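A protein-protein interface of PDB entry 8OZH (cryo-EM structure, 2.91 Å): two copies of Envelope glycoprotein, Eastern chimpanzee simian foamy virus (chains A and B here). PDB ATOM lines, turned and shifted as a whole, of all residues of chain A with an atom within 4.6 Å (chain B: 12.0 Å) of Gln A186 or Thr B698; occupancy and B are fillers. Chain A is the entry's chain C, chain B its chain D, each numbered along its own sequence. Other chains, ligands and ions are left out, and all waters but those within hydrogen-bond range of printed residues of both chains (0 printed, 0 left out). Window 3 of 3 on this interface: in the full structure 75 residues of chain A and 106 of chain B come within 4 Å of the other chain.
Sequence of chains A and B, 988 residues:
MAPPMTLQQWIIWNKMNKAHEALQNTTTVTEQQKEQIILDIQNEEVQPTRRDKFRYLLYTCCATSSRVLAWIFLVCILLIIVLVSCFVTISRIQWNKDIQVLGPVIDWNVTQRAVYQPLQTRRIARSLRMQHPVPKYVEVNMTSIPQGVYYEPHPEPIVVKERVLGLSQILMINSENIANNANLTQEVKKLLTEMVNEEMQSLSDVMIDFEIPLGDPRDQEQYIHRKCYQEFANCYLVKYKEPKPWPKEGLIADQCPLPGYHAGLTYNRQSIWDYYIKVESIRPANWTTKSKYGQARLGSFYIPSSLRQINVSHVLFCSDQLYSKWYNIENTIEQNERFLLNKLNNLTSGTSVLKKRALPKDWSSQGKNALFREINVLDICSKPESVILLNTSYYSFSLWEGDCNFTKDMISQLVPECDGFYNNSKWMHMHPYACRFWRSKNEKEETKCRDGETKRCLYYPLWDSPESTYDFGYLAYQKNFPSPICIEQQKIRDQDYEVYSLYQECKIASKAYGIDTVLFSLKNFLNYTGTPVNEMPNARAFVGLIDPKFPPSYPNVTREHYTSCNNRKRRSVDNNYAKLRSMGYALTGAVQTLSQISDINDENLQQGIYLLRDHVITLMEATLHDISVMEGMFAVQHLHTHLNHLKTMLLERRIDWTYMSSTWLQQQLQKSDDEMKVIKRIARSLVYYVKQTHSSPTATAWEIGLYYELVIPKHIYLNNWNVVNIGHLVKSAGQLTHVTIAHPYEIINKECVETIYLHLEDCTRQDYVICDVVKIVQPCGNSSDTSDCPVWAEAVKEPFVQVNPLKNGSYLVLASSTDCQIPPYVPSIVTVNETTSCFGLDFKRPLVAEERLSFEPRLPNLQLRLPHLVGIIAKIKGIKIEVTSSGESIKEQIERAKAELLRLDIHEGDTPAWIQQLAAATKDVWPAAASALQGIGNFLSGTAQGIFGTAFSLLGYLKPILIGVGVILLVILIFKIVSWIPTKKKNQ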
ATOM      1  N   SER A 175      26.387 -30.908  31.629  1.00  0.00           N
ATOM      2  CA  SER A 175      24.919 -30.778  31.825  1.00  0.00           C
ATOM      3  C   SER A 175      24.236 -32.147  31.678  1.00  0.00           C
ATOM      4  O   SER A 175      23.358 -32.449  32.530  1.00  0.00           O
ATOM      5  CB  SER A 175      24.327 -29.736  30.905  1.00  0.00           C
ATOM      6  OG  SER A 175      24.394 -30.145  29.546  1.00  0.00           O
ATOM      7  N   LEU A 184      15.015 -34.918  33.580  1.00  0.00           N
ATOM      8  CA  LEU A 184      14.581 -33.679  32.877  1.00  0.00           C
ATOM      9  C   LEU A 184      14.005 -34.025  31.500  1.00  0.00           C
ATOM     10  O   LEU A 184      14.338 -35.099  30.975  1.00  0.00           O
ATOM     11  CB  LEU A 184      15.758 -32.710  32.735  1.00  0.00           C
ATOM     12  CG  LEU A 184      16.366 -32.171  34.028  1.00  0.00           C
ATOM     13  CD1 LEU A 184      17.365 -31.063  33.728  1.00  0.00           C
ATOM     14  CD2 LEU A 184      15.300 -31.660  34.976  1.00  0.00           C
ATOM     15  N   THR A 185      13.188 -33.121  30.948  1.00  0.00           N
ATOM     16  CA  THR A 185      12.586 -33.195  29.588  1.00  0.00           C
ATOM     17  C   THR A 185      13.342 -32.265  28.630  1.00  0.00           C
ATOM     18  O   THR A 185      13.996 -31.306  29.116  1.00  0.00           O
ATOM     19  CB  THR A 185      11.096 -32.832  29.618  1.00  0.00           C
ATOM     20  OG1 THR A 185      10.945 -31.413  29.683  1.00  0.00           O
ATOM     21  CG2 THR A 185      10.364 -33.463  30.783  1.00  0.00           C
ATOM     22  N   GLN A 186      13.188 -32.492  27.321  1.00  0.00           N
ATOM     23  CA  GLN A 186      13.945 -31.789  26.247  1.00  0.00           C
ATOM     24  C   GLN A 186      13.693 -30.276  26.310  1.00  0.00           C
ATOM     25  O   GLN A 186      14.573 -29.526  25.844  1.00  0.00           O
ATOM     26  CB  GLN A 186      13.582 -32.329  24.860  1.00  0.00           C
ATOM     27  CG  GLN A 186      13.934 -33.799  24.649  1.00  0.00           C
ATOM     28  CD  GLN A 186      15.410 -34.084  24.789  1.00  0.00           C
ATOM     29  OE1 GLN A 186      16.244 -33.481  24.117  1.00  0.00           O
ATOM     30  NE2 GLN A 186      15.745 -35.016  25.669  1.00  0.00           N
ATOM     31  N   GLU A 187      12.545 -29.843  26.842  1.00  0.00           N
ATOM     32  CA  GLU A 187      12.232 -28.409  27.082  1.00  0.00           C
ATOM     33  C   GLU A 187      13.101 -27.866  28.225  1.00  0.00           C
ATOM     34  O   GLU A 187      13.639 -26.754  28.076  1.00  0.00           O
ATOM     35  CB  GLU A 187      10.749 -28.217  27.399  1.00  0.00           C
ATOM     36  CG  GLU A 187       9.842 -28.415  26.195  1.00  0.00           C
ATOM     37  CD  GLU A 187       8.395 -27.980  26.380  1.00  0.00           C
ATOM     38  OE1 GLU A 187       8.139 -27.079  27.213  1.00  0.00           O
ATOM     39  OE2 GLU A 187       7.518 -28.542  25.684  1.00  0.00           O
ATOM     40  N   VAL A 188      13.236 -28.616  29.320  1.00  0.00           N
ATOM     41  CA  VAL A 188      13.934 -28.146  30.554  1.00  0.00           C
ATOM     42  C   VAL A 188      15.450 -28.267  30.335  1.00  0.00           C
ATOM     43  O   VAL A 188      16.207 -27.366  30.819  1.00  0.00           O
ATOM     44  CB  VAL A 188      13.439 -28.907  31.800  1.00  0.00           C
ATOM     45  CG1 VAL A 188      14.078 -28.397  33.084  1.00  0.00           C
ATOM     46  CG2 VAL A 188      11.926 -28.841  31.913  1.00  0.00           C
ATOM     47  N   LYS A 189      15.889 -29.302  29.607  1.00  0.00           N
ATOM     48  CA  LYS A 189      17.295 -29.435  29.129  1.00  0.00           C
ATOM     49  C   LYS A 189      17.757 -28.110  28.503  1.00  0.00           C
ATOM     50  O   LYS A 189      18.892 -27.693  28.806  1.00  0.00           O
ATOM     51  CB  LYS A 189      17.447 -30.599  28.144  1.00  0.00           C
ATOM     52  CG  LYS A 189      17.487 -31.977  28.790  1.00  0.00           C
ATOM     53  CD  LYS A 189      18.088 -33.038  27.900  1.00  0.00           C
ATOM     54  CE  LYS A 189      18.088 -34.409  28.542  1.00  0.00           C
ATOM     55  NZ  LYS A 189      18.623 -35.452  27.633  1.00  0.00           N
ATOM     56  N   LYS A 190      16.908 -27.452  27.704  1.00  0.00           N
ATOM     57  CA  LYS A 190      17.232 -26.141  27.078  1.00  0.00           C
ATOM     58  C   LYS A 190      17.402 -25.060  28.153  1.00  0.00           C
ATOM     59  O   LYS A 190      18.259 -24.181  27.954  1.00  0.00           O
ATOM     60  CB  LYS A 190      16.170 -25.715  26.064  1.00  0.00           C
ATOM     61  CG  LYS A 190      16.204 -26.470  24.745  1.00  0.00           C
ATOM     62  CD  LYS A 190      15.660 -25.669  23.582  1.00  0.00           C
ATOM     63  CE  LYS A 190      15.836 -26.371  22.252  1.00  0.00           C
ATOM     64  NZ  LYS A 190      15.853 -25.409  21.121  1.00  0.00           N
ATOM     65  N   THR A 193      20.748 -25.626  30.067  1.00  0.00           N
ATOM     66  CA  THR A 193      21.881 -25.304  29.160  1.00  0.00           C
ATOM     67  C   THR A 193      22.086 -23.787  29.085  1.00  0.00           C
ATOM     68  O   THR A 193      23.254 -23.348  29.197  1.00  0.00           O
ATOM     69  CB  THR A 193      21.674 -25.939  27.783  1.00  0.00           C
ATOM     70  OG1 THR A 193      21.567 -27.346  27.996  1.00  0.00           O
ATOM     71  CG2 THR A 193      22.813 -25.666  26.826  1.00  0.00           C
ATOM     72  N   GLU A 535      23.143 -37.726  23.865  1.00  0.00           N
ATOM     73  CA  GLU A 535      22.235 -36.575  24.135  1.00  0.00           C
ATOM     74  C   GLU A 535      20.753 -36.986  24.050  1.00  0.00           C
ATOM     75  O   GLU A 535      19.900 -36.130  24.369  1.00  0.00           O
ATOM     76  CB  GLU A 535      22.546 -35.431  23.171  1.00  0.00           C
ATOM     77  CG  GLU A 535      23.880 -34.761  23.452  1.00  0.00           C
ATOM     78  CD  GLU A 535      24.303 -33.731  22.416  1.00  0.00           C
ATOM     79  OE1 GLU A 535      23.421 -32.996  21.913  1.00  0.00           O
ATOM     80  OE2 GLU A 535      25.513 -33.670  22.108  1.00  0.00           O
ATOM     81  N   PRO A 537      17.274 -39.058  25.401  1.00  0.00           N
ATOM     82  CA  PRO A 537      16.768 -39.405  26.732  1.00  0.00           C
ATOM     83  C   PRO A 537      17.088 -40.845  27.160  1.00  0.00           C
ATOM     84  O   PRO A 537      16.933 -41.743  26.348  1.00  0.00           O
ATOM     85  CB  PRO A 537      15.249 -39.211  26.645  1.00  0.00           C
ATOM     86  CG  PRO A 537      14.937 -39.205  25.163  1.00  0.00           C
ATOM     87  CD  PRO A 537      16.189 -38.713  24.472  1.00  0.00           C
ATOM     88  N   GLY B 632      13.204 -32.096  38.052  1.00  0.00           N
ATOM     89  CA  GLY B 632      12.645 -31.007  37.227  1.00  0.00           C
ATOM     90  C   GLY B 632      13.334 -29.678  37.484  1.00  0.00           C
ATOM     91  O   GLY B 632      14.561 -29.683  37.708  1.00  0.00           O
ATOM     92  N   MET B 633      12.571 -28.579  37.466  1.00  0.00           N
ATOM     93  CA  MET B 633      13.094 -27.196  37.640  1.00  0.00           C
ATOM     94  C   MET B 633      13.663 -27.003  39.056  1.00  0.00           C
ATOM     95  O   MET B 633      14.552 -26.130  39.207  1.00  0.00           O
ATOM     96  CB  MET B 633      12.007 -26.148  37.375  1.00  0.00           C
ATOM     97  CG  MET B 633      11.758 -25.858  35.903  1.00  0.00           C
ATOM     98  SD  MET B 633      13.180 -25.111  35.036  1.00  0.00           S
ATOM     99  CE  MET B 633      13.396 -23.571  35.929  1.00  0.00           C
ATOM    100  N   VAL B 636      17.193 -27.683  38.772  1.00  0.00           N
ATOM    101  CA  VAL B 636      17.813 -26.610  37.941  1.00  0.00           C
ATOM    102  C   VAL B 636      18.047 -25.361  38.802  1.00  0.00           C
ATOM    103  O   VAL B 636      19.166 -24.809  38.735  1.00  0.00           O
ATOM    104  CB  VAL B 636      16.964 -26.299  36.693  1.00  0.00           C
ATOM    105  CG1 VAL B 636      17.480 -25.079  35.946  1.00  0.00           C
ATOM    106  CG2 VAL B 636      16.881 -27.492  35.754  1.00  0.00           C
ATOM    107  N   LEU B 639      21.028 -25.659  41.437  1.00  0.00           N
ATOM    108  CA  LEU B 639      22.349 -25.552  40.759  1.00  0.00           C
ATOM    109  C   LEU B 639      22.663 -24.075  40.452  1.00  0.00           C
ATOM    110  O   LEU B 639      23.805 -23.629  40.720  1.00  0.00           O
ATOM    111  CB  LEU B 639      22.328 -26.415  39.492  1.00  0.00           C
ATOM    112  CG  LEU B 639      23.622 -26.446  38.670  1.00  0.00           C
ATOM    113  CD1 LEU B 639      24.797 -26.975  39.478  1.00  0.00           C
ATOM    114  CD2 LEU B 639      23.436 -27.279  37.412  1.00  0.00           C
ATOM    115  N   GLN B 692      35.230 -23.720  27.437  1.00  0.00           N
ATOM    116  CA  GLN B 692      34.001 -24.471  27.056  1.00  0.00           C
ATOM    117  C   GLN B 692      34.400 -25.642  26.151  1.00  0.00           C
ATOM    118  O   GLN B 692      34.916 -25.380  25.057  1.00  0.00           O
ATOM    119  CB  GLN B 692      32.975 -23.567  26.372  1.00  0.00           C
ATOM    120  CG  GLN B 692      31.769 -24.336  25.842  1.00  0.00           C
ATOM    121  CD  GLN B 692      30.574 -23.456  25.575  1.00  0.00           C
ATOM    122  OE1 GLN B 692      30.706 -22.301  25.182  1.00  0.00           O
ATOM    123  NE2 GLN B 692      29.388 -24.003  25.777  1.00  0.00           N
ATOM    124  N   HIS B 694      32.368 -28.348  25.033  1.00  0.00           N
ATOM    125  CA  HIS B 694      31.277 -28.879  24.167  1.00  0.00           C
ATOM    126  C   HIS B 694      30.078 -27.928  24.196  1.00  0.00           C
ATOM    127  O   HIS B 694      29.773 -27.433  25.285  1.00  0.00           O
ATOM    128  CB  HIS B 694      30.881 -30.288  24.624  1.00  0.00           C
ATOM    129  CG  HIS B 694      29.771 -30.889  23.827  1.00  0.00           C
ATOM    130  ND1 HIS B 694      28.443 -30.755  24.192  1.00  0.00           N
ATOM    131  CD2 HIS B 694      29.780 -31.615  22.686  1.00  0.00           C
ATOM    132  CE1 HIS B 694      27.684 -31.370  23.308  1.00  0.00           C
ATOM    133  NE2 HIS B 694      28.480 -31.909  22.376  1.00  0.00           N
ATOM    134  N   SER B 695      29.410 -27.717  23.058  1.00  0.00           N
ATOM    135  CA  SER B 695      28.295 -26.740  22.908  1.00  0.00           C
ATOM    136  C   SER B 695      27.260 -27.219  21.880  1.00  0.00           C
ATOM    137  O   SER B 695      27.428 -26.920  20.682  1.00  0.00           O
ATOM    138  CB  SER B 695      28.832 -25.380  22.550  1.00  0.00           C
ATOM    139  OG  SER B 695      27.777 -24.447  22.376  1.00  0.00           O
ATOM    140  N   SER B 696      26.220 -27.912  22.351  1.00  0.00           N
ATOM    141  CA  SER B 696      24.990 -28.277  21.596  1.00  0.00           C
ATOM    142  C   SER B 696      23.855 -27.356  22.047  1.00  0.00           C
ATOM    143  O   SER B 696      23.996 -26.659  23.050  1.00  0.00           O
ATOM    144  CB  SER B 696      24.669 -29.747  21.804  1.00  0.00           C
ATOM    145  OG  SER B 696      23.273 -30.010  21.752  1.00  0.00           O
ATOM    146  N   PRO B 697      22.716 -27.274  21.322  1.00  0.00           N
ATOM    147  CA  PRO B 697      21.529 -26.578  21.834  1.00  0.00           C
ATOM    148  C   PRO B 697      20.873 -27.168  23.099  1.00  0.00           C
ATOM    149  O   PRO B 697      20.184 -26.424  23.773  1.00  0.00           O
ATOM    150  CB  PRO B 697      20.545 -26.633  20.652  1.00  0.00           C
ATOM    151  CG  PRO B 697      21.034 -27.787  19.809  1.00  0.00           C
ATOM    152  CD  PRO B 697      22.539 -27.719  19.930  1.00  0.00           C
ATOM    153  N   THR B 698      21.084 -28.453  23.396  1.00  0.00           N
ATOM    154  CA  THR B 698      20.545 -29.139  24.605  1.00  0.00           C
ATOM    155  C   THR B 698      21.649 -29.469  25.615  1.00  0.00           C
ATOM    156  O   THR B 698      21.277 -29.814  26.756  1.00  0.00           O
ATOM    157  CB  THR B 698      19.807 -30.437  24.250  1.00  0.00           C
ATOM    158  OG1 THR B 698      20.537 -31.114  23.223  1.00  0.00           O
ATOM    159  CG2 THR B 698      18.384 -30.199  23.798  1.00  0.00           C
ATOM    160  N   ALA B 699      22.935 -29.389  25.246  1.00  0.00           N
ATOM    161  CA  ALA B 699      24.060 -29.838  26.105  1.00  0.00           C
ATOM    162  C   ALA B 699      25.223 -28.835  26.086  1.00  0.00           C
ATOM    163  O   ALA B 699      25.459 -28.233  25.028  1.00  0.00           O
ATOM    164  CB  ALA B 699      24.491 -31.208  25.657  1.00  0.00           C
ATOM    165  N   THR B 700      25.900 -28.655  27.227  1.00  0.00           N
ATOM    166  CA  THR B 700      27.188 -27.916  27.365  1.00  0.00           C
ATOM    167  C   THR B 700      28.136 -28.640  28.320  1.00  0.00           C
ATOM    168  O   THR B 700      27.668 -29.475  29.123  1.00  0.00           O
ATOM    169  CB  THR B 700      27.036 -26.498  27.930  1.00  0.00           C
ATOM    170  OG1 THR B 700      26.283 -26.542  29.145  1.00  0.00           O
ATOM    171  CG2 THR B 700      26.376 -25.557  26.949  1.00  0.00           C
ATOM    172  N   ALA B 701      29.415 -28.277  28.254  1.00  0.00           N
ATOM    173  CA  ALA B 701      30.461 -28.702  29.203  1.00  0.00           C
ATOM    174  C   ALA B 701      31.533 -27.613  29.309  1.00  0.00           C
ATOM    175  O   ALA B 701      31.904 -27.033  28.262  1.00  0.00           O
ATOM    176  CB  ALA B 701      31.019 -30.010  28.735  1.00  0.00           C
ATOM    177  N   TRP B 702      32.010 -27.347  30.525  1.00  0.00           N
ATOM    178  CA  TRP B 702      33.078 -26.357  30.811  1.00  0.00           C
ATOM    179  C   TRP B 702      34.168 -26.994  31.679  1.00  0.00           C
ATOM    180  O   TRP B 702      33.877 -27.981  32.357  1.00  0.00           O
ATOM    181  CB  TRP B 702      32.486 -25.113  31.487  1.00  0.00           C
ATOM    182  CG  TRP B 702      31.554 -24.305  30.635  1.00  0.00           C
ATOM    183  CD1 TRP B 702      30.262 -24.601  30.311  1.00  0.00           C
ATOM    184  CD2 TRP B 702      31.838 -23.043  30.013  1.00  0.00           C
ATOM    185  NE1 TRP B 702      29.726 -23.618  29.523  1.00  0.00           N
ATOM    186  CE2 TRP B 702      30.667 -22.648  29.326  1.00  0.00           C
ATOM    187  CE3 TRP B 702      32.963 -22.209  29.971  1.00  0.00           C
ATOM    188  CZ2 TRP B 702      30.594 -21.456  28.609  1.00  0.00           C
ATOM    189  CZ3 TRP B 702      32.890 -21.026  29.264  1.00  0.00           C
ATOM    190  CH2 TRP B 702      31.721 -20.659  28.589  1.00  0.00           C
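Of the 11 printed residues of chain A, 7 touch a printed residue of chain B.
Printed residues of chain A that touch a printed residue of chain B: Ser A175, Leu A184, Gln A186, Val A188, Lys A189, Thr A193 and Glu A535.
Hydrophobic or aromatic side chains of chain A that line the printed part of chain B: Leu A184 and Val A188.
Of the 14 printed residues of chain B, 8 touch a printed residue of chain A.
Hydrophobic or aromatic side chains of chain B that line the printed part of chain A: Met B633, Val B636 and His B694.
Among the printed residues, no Asp or Glu carboxylate lies within 4 Å of a Lys or Arg side-chain nitrogen of the other chain.
No position is printed for both chains.
O of Lys A189 sits at hydrogen-bond distance from OG1 of Thr A193, at 2.8 Å.
The side-chain amide nitrogen of Gln B692 lies within hydrogen-bond range of the backbone carbonyl oxygen of His B694 (3.5 Å).
The backbone carbonyl oxygen (O) of His B694 is in hydrogen-bond range of the backbone NH (N) of Ala B701 (3.1 Å).
N of Thr B698 lies within hydrogen-bond range of OG of Ser B696 (3.1 Å).
Among the printed residues, merely in contact across the chains: Ser A175 with Ala B699 (3.5 Å), Leu A184 with Gly B632 (3.5 Å), Gln A186 with Thr B698 (3.9 Å), Val A188 with Met B633 (3.9 Å), Val A188 with Val B636 (3.98 Å), Lys A189 with Thr B698 (3.8 Å), Thr A193 with Ala B699 (3.7 Å), Thr A193 with Thr B700 (3.6 Å) and Glu A535 with Thr B698 (3.7 Å).
N of Thr B700 lies within hydrogen-bond range of OG of Ser A175 (3.1 Å).
The side-chain hydroxyl (OG1) of Thr A193 sits at hydrogen-bond distance from the backbone carbonyl oxygen (O) of Thr B698 (2.8 Å).
NE2 of His B694 lies close to OE2 of Glu A535 (3.5 Å).
OG of Ser B696 lies within hydrogen-bond range of OE1 of Glu A535, at 3.0 Å.
Gln A186 touches just one residue of chain B: Thr B698.
Ser A175 touches just these residues of chain B: Ala B699 and Thr B700.
No residue of chain B comes within 4 Å of Glu A187.
Of the printed residues of chain B, Val A188 touches Met B633 and Val B636.
Of chain B, only Thr B698 comes within 4 Å of Lys A189.
No residue of chain B comes within 4 Å of Lys A190.
Thr A193 touches three residues of chain B.
No residue of chain B comes within 4 Å of Pro A537.
Of the printed residues of chain A, Val B636 touches Val A188.
Of the printed residues of chain A, Gly B632 touches Leu A184.
Of the printed residues of chain A, Met B633 touches Val A188.
Of the printed residues of chain A, Ala B699 touches Ser A175 (3.5 Å) and Thr A193 (3.7 Å).
Printed residues of chain B within 4 Å of Leu A184: Gly B632 (3.5 Å).
The nearest residue of chain B that does not touch Gln A186 is Pro B697 (6.7 Å).
The nearest residue of chain A that does not touch Thr B698 is Ser A175 (4.2 Å).
The nearest printed residue of chain A that does not touch His B694 is Ser A175 (6.7 Å).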
